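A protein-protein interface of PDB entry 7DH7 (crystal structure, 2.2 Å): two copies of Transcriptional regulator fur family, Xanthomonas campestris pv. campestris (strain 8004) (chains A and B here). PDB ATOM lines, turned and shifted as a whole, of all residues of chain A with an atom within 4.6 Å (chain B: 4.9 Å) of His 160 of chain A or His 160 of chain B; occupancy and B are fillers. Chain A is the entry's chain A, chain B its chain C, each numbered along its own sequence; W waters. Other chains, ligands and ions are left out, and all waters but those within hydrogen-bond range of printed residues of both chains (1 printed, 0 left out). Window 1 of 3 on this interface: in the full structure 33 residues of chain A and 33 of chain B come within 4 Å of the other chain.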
ATOM      1  N   ILE A 122       5.154  -7.426  14.599  1.00  0.00           N
ATOM      2  CA  ILE A 122       5.225  -8.324  13.452  1.00  0.00           C
ATOM      3  C   ILE A 122       5.859  -9.648  13.863  1.00  0.00           C
ATOM      4  O   ILE A 122       6.861  -9.673  14.594  1.00  0.00           O
ATOM      5  CB  ILE A 122       6.028  -7.675  12.301  1.00  0.00           C
ATOM      6  CG1 ILE A 122       5.494  -6.277  11.979  1.00  0.00           C
ATOM      7  CG2 ILE A 122       6.049  -8.550  11.043  1.00  0.00           C
ATOM      8  CD1 ILE A 122       6.525  -5.215  12.273  1.00  0.00           C
ATOM      9  N   ASP A 124       8.063 -12.946  13.101  1.00  0.00           N
ATOM     10  CA  ASP A 124       9.244 -13.335  12.310  1.00  0.00           C
ATOM     11  C   ASP A 124       8.941 -14.409  11.284  1.00  0.00           C
ATOM     12  O   ASP A 124       9.650 -14.531  10.279  1.00  0.00           O
ATOM     13  CB  ASP A 124      10.326 -13.920  13.224  1.00  0.00           C
ATOM     14  CG  ASP A 124      11.252 -12.908  13.735  1.00  0.00           C
ATOM     15  OD1 ASP A 124      11.169 -11.769  13.232  1.00  0.00           O
ATOM     16  OD2 ASP A 124      12.049 -13.248  14.646  1.00  0.00           O
ATOM     17  N   LEU A 157       8.671   3.095  14.743  1.00  0.00           N
ATOM     18  CA  LEU A 157       9.312   1.872  15.203  1.00  0.00           C
ATOM     19  C   LEU A 157       8.512   0.624  14.808  1.00  0.00           C
ATOM     20  O   LEU A 157       7.295   0.664  14.597  1.00  0.00           O
ATOM     21  CB  LEU A 157       9.475   1.908  16.723  1.00  0.00           C
ATOM     22  CG  LEU A 157      10.340   3.026  17.320  1.00  0.00           C
ATOM     23  CD1 LEU A 157      10.303   2.957  18.841  1.00  0.00           C
ATOM     24  CD2 LEU A 157      11.784   2.975  16.800  1.00  0.00           C
ATOM     25  N   GLU A 158       9.219  -0.507  14.735  1.00  0.00           N
ATOM     26  CA  GLU A 158       8.587  -1.812  14.595  1.00  0.00           C
ATOM     27  C   GLU A 158       9.070  -2.720  15.714  1.00  0.00           C
ATOM     28  O   GLU A 158      10.243  -2.675  16.097  1.00  0.00           O
ATOM     29  CB  GLU A 158       8.907  -2.452  13.236  1.00  0.00           C
ATOM     30  CG  GLU A 158       8.120  -1.851  12.098  1.00  0.00           C
ATOM     31  CD  GLU A 158       8.373  -2.538  10.764  1.00  0.00           C
ATOM     32  OE1 GLU A 158       9.428  -3.182  10.568  1.00  0.00           O
ATOM     33  OE2 GLU A 158       7.499  -2.423   9.909  1.00  0.00           O
ATOM     34  N   VAL A 159       8.158  -3.540  16.234  1.00  0.00           N
ATOM     35  CA  VAL A 159       8.479  -4.591  17.192  1.00  0.00           C
ATOM     36  C   VAL A 159       8.394  -5.928  16.462  1.00  0.00           C
ATOM     37  O   VAL A 159       7.421  -6.190  15.743  1.00  0.00           O
ATOM     38  CB  VAL A 159       7.535  -4.539  18.403  1.00  0.00           C
ATOM     39  CG1 VAL A 159       7.961  -5.522  19.464  1.00  0.00           C
ATOM     40  CG2 VAL A 159       7.474  -3.125  18.960  1.00  0.00           C
ATOM     41  N   HIS A 160       9.426  -6.753  16.605  1.00  0.00           N
ATOM     42  CA  HIS A 160       9.509  -8.030  15.903  1.00  0.00           C
ATOM     43  C   HIS A 160       9.574  -9.142  16.934  1.00  0.00           C
ATOM     44  O   HIS A 160      10.404  -9.104  17.847  1.00  0.00           O
ATOM     45  CB  HIS A 160      10.729  -8.086  14.977  1.00  0.00           C
ATOM     46  CG  HIS A 160      10.638  -7.166  13.801  1.00  0.00           C
ATOM     47  ND1 HIS A 160      10.649  -7.614  12.501  1.00  0.00           N
ATOM     48  CD2 HIS A 160      10.494  -5.822  13.732  1.00  0.00           C
ATOM     49  CE1 HIS A 160      10.535  -6.586  11.679  1.00  0.00           C
ATOM     50  NE2 HIS A 160      10.437  -5.486  12.400  1.00  0.00           N
ATOM     51  N   GLY A 161       8.694 -10.122  16.792  1.00  0.00           N
ATOM     52  CA  GLY A 161       8.627 -11.212  17.737  1.00  0.00           C
ATOM     53  C   GLY A 161       8.070 -12.444  17.067  1.00  0.00           C
ATOM     54  O   GLY A 161       8.164 -12.586  15.842  1.00  0.00           O
ATOM     55  N   LEU B 121      17.318  -3.034  20.520  1.00  0.00           N
ATOM     56  CA  LEU B 121      16.828  -1.925  19.678  1.00  0.00           C
ATOM     57  C   LEU B 121      17.884  -1.720  18.585  1.00  0.00           C
ATOM     58  O   LEU B 121      18.994  -1.378  18.949  1.00  0.00           O
ATOM     59  CB  LEU B 121      16.696  -0.725  20.611  1.00  0.00           C
ATOM     60  CG  LEU B 121      16.217   0.573  19.989  1.00  0.00           C
ATOM     61  CD1 LEU B 121      14.931   0.352  19.217  1.00  0.00           C
ATOM     62  CD2 LEU B 121      16.010   1.613  21.068  1.00  0.00           C
ATOM     63  N   ILE B 122      17.491  -2.049  17.371  1.00  0.00           N
ATOM     64  CA  ILE B 122      18.438  -2.111  16.245  1.00  0.00           C
ATOM     65  C   ILE B 122      18.119  -1.059  15.204  1.00  0.00           C
ATOM     66  O   ILE B 122      16.983  -0.867  14.917  1.00  0.00           O
ATOM     67  CB  ILE B 122      18.401  -3.531  15.662  1.00  0.00           C
ATOM     68  CG1 ILE B 122      18.659  -4.583  16.734  1.00  0.00           C
ATOM     69  CG2 ILE B 122      19.367  -3.662  14.513  1.00  0.00           C
ATOM     70  CD1 ILE B 122      17.481  -5.415  17.063  1.00  0.00           C
ATOM     71  N   THR B 156      12.431 -13.357  22.701  1.00  0.00           N
ATOM     72  CA  THR B 156      12.541 -11.991  23.188  1.00  0.00           C
ATOM     73  C   THR B 156      12.298 -11.010  22.043  1.00  0.00           C
ATOM     74  O   THR B 156      12.696 -11.248  20.897  1.00  0.00           O
ATOM     75  CB  THR B 156      13.916 -11.774  23.826  1.00  0.00           C
ATOM     76  OG1 THR B 156      14.163 -12.832  24.758  1.00  0.00           O
ATOM     77  CG2 THR B 156      13.979 -10.439  24.574  1.00  0.00           C
ATOM     78  N   LEU B 157      11.597  -9.923  22.351  1.00  0.00           N
ATOM     79  CA  LEU B 157      11.242  -8.959  21.324  1.00  0.00           C
ATOM     80  C   LEU B 157      12.476  -8.213  20.832  1.00  0.00           C
ATOM     81  O   LEU B 157      13.454  -8.018  21.568  1.00  0.00           O
ATOM     82  CB  LEU B 157      10.217  -7.962  21.857  1.00  0.00           C
ATOM     83  CG  LEU B 157       8.884  -8.578  22.251  1.00  0.00           C
ATOM     84  CD1 LEU B 157       8.020  -7.519  22.915  1.00  0.00           C
ATOM     85  CD2 LEU B 157       8.204  -9.139  21.014  1.00  0.00           C
ATOM     86  N   GLU B 158      12.423  -7.804  19.565  1.00  0.00           N
ATOM     87  CA  GLU B 158      13.348  -6.829  19.009  1.00  0.00           C
ATOM     88  C   GLU B 158      12.560  -5.598  18.586  1.00  0.00           C
ATOM     89  O   GLU B 158      11.414  -5.708  18.122  1.00  0.00           O
ATOM     90  CB  GLU B 158      14.130  -7.384  17.808  1.00  0.00           C
ATOM     91  CG  GLU B 158      15.134  -8.456  18.161  1.00  0.00           C
ATOM     92  CD  GLU B 158      16.122  -8.747  17.041  1.00  0.00           C
ATOM     93  OE1 GLU B 158      15.914  -8.257  15.905  1.00  0.00           O
ATOM     94  OE2 GLU B 158      17.112  -9.458  17.304  1.00  0.00           O
ATOM     95  N   VAL B 159      13.163  -4.426  18.753  1.00  0.00           N
ATOM     96  CA  VAL B 159      12.578  -3.178  18.284  1.00  0.00           C
ATOM     97  C   VAL B 159      13.471  -2.639  17.188  1.00  0.00           C
ATOM     98  O   VAL B 159      14.696  -2.589  17.346  1.00  0.00           O
ATOM     99  CB  VAL B 159      12.397  -2.161  19.422  1.00  0.00           C
ATOM    100  CG1 VAL B 159      11.740  -0.884  18.901  1.00  0.00           C
ATOM    101  CG2 VAL B 159      11.562  -2.777  20.527  1.00  0.00           C
ATOM    102  N   HIS B 160      12.852  -2.310  16.062  1.00  0.00           N
ATOM    103  CA  HIS B 160      13.600  -1.841  14.876  1.00  0.00           C
ATOM    104  C   HIS B 160      13.236  -0.400  14.573  1.00  0.00           C
ATOM    105  O   HIS B 160      12.076  -0.091  14.523  1.00  0.00           O
ATOM    106  CB  HIS B 160      13.429  -2.771  13.673  1.00  0.00           C
ATOM    107  CG  HIS B 160      13.939  -4.147  13.878  1.00  0.00           C
ATOM    108  ND1 HIS B 160      14.701  -4.770  12.958  1.00  0.00           N
ATOM    109  CD2 HIS B 160      13.793  -5.023  14.883  1.00  0.00           C
ATOM    110  CE1 HIS B 160      15.001  -5.966  13.377  1.00  0.00           C
ATOM    111  NE2 HIS B 160      14.472  -6.141  14.544  1.00  0.00           N
ATOM    112  N   GLY B 161      14.260   0.401  14.357  1.00  0.00           N
ATOM    113  CA  GLY B 161      14.127   1.834  14.123  1.00  0.00           C
ATOM    114  C   GLY B 161      15.276   2.374  13.323  1.00  0.00           C
ATOM    115  O   GLY B 161      16.054   1.580  12.797  1.00  0.00           O
ATOM    116  N   LEU B 162      15.295   3.685  13.160  1.00  0.00           N
ATOM    117  CA  LEU B 162      16.383   4.358  12.432  1.00  0.00           C
ATOM    118  C   LEU B 162      17.177   5.209  13.433  1.00  0.00           C
ATOM    119  O   LEU B 162      16.553   6.012  14.117  1.00  0.00           O
ATOM    120  CB  LEU B 162      15.745   5.209  11.340  1.00  0.00           C
ATOM    121  CG  LEU B 162      16.720   5.923  10.415  1.00  0.00           C
ATOM    122  CD1 LEU B 162      17.598   4.915   9.700  1.00  0.00           C
ATOM    123  CD2 LEU B 162      15.964   6.761   9.402  1.00  0.00           C
HETATM  124  O   HOH W   1      12.359 -10.990  18.343  1.00  0.00           O
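The backbone carbonyl oxygen (O) of Glu 158 of chain A lies within hydrogen-bond range of the backbone NH (N) of His 160 of chain B (2.6 Å). O of Glu 158 of chain B is in hydrogen-bond range of N of His 160 of chain A.
Leu 157 of chain A touches Gly 161 of chain B, and with the chains exchanged Gly 161 of chain A touches Leu 157 of chain B. Glu 158 of chain A touches Val 159 of chain B, and with the chains exchanged Val 159 of chain A touches Glu 158 of chain B. Val 159 of chain A touches Leu 157 of chain B, but with the chains exchanged Leu 157 of chain A does not touch Val 159 of chain B (4.1 Å). His 160 of chain B touches its own counterpart, His 160 of chain A. Of the 11 pairs that touch across the chains among the printed residues, 10 have their exchanged pair printed and touching as well.
Of the 9 printed residues of chain B, 5 touch a printed residue of chain A. Hydrophobic or aromatic side chains of chain B within 4 Å of the printed part of chain A: Leu 157, Val 159 and His 160. Along chain B the printed residues that touch a printed residue of chain A span positions 157 to 161. Hydrophobic or aromatic side chains of chain A within 4 Å of the printed part of chain B: Leu 157, Val 159 and His 160. Among the printed residues, 11 pairs touch across the chains.
His 160 of chain A touches three residues of chain B. Printed residues of chain B within 4 Å of Glu 158 of chain A: Glu 158, Val 159 and His 160. Printed residues of chain B within 4 Å of Val 159 of chain A: Leu 157 and Glu 158. Printed residues of chain B within 4 Å of Gly 161 of chain A: Leu 157. Of the printed residues of chain A, Glu 158 of chain B touches Glu 158, Val 159 and His 160. Thr 156 of chain B touches none of the printed residues of chain A. The nearest printed residue of chain A that does not touch His 160 of chain B is Val 159 of chain A (4.9 Å).
Water W1 lies within hydrogen-bond range of O of Thr 156 of chain B, O of His 160 of chain A and N of Glu 158 of chain B.
CA of Leu 157 of chain A touches O of His 160 of chain B (3.5 Å). Gly 161 of chain B touches Leu 157 of chain A (CA to CD2, 3.7 Å). Glu 158 of chain A touches Glu 158 of chain B. O of Glu 158 of chain A touches CA of Val 159 of chain B, at 3.2 Å. CD2 of Leu 157 of chain B touches CG1 of Val 159 of chain A, at 3.9 Å. Val 159 of chain A touches Glu 158 of chain B (CA to O, 3.3 Å). Leu 157 of chain B touches His 160 of chain A. His 160 of chain B touches His 160 of chain A (CD2 to CD2, 3.6 Å). Gly 161 of chain A touches Leu 157 of chain B (CA to CD2, 3.9 Å).
The backbone NH of Ile 122 of chain A lies within hydrogen-bond range of the backbone carbonyl oxygen of Val 159 of chain A, at 2.8 Å. O of Ile 122 of chain A lies within hydrogen-bond range of N of Gly 161 of chain A (2.9 Å). The backbone carbonyl oxygen of Gly 161 of chain A is in hydrogen-bond range of the backbone NH of Asp 124 of chain A. The backbone NH (N) of Ile 122 of chain B sits at hydrogen-bond distance from the backbone carbonyl oxygen (O) of Val 159 of chain B. O of Ile 122 of chain B lies within hydrogen-bond range of N of Gly 161 of chain B. The side-chain carboxylate (OE1) of Glu 158 of chain B sits at hydrogen-bond distance from a ring nitrogen (NE2) of His 160 of chain B (2.9 Å).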
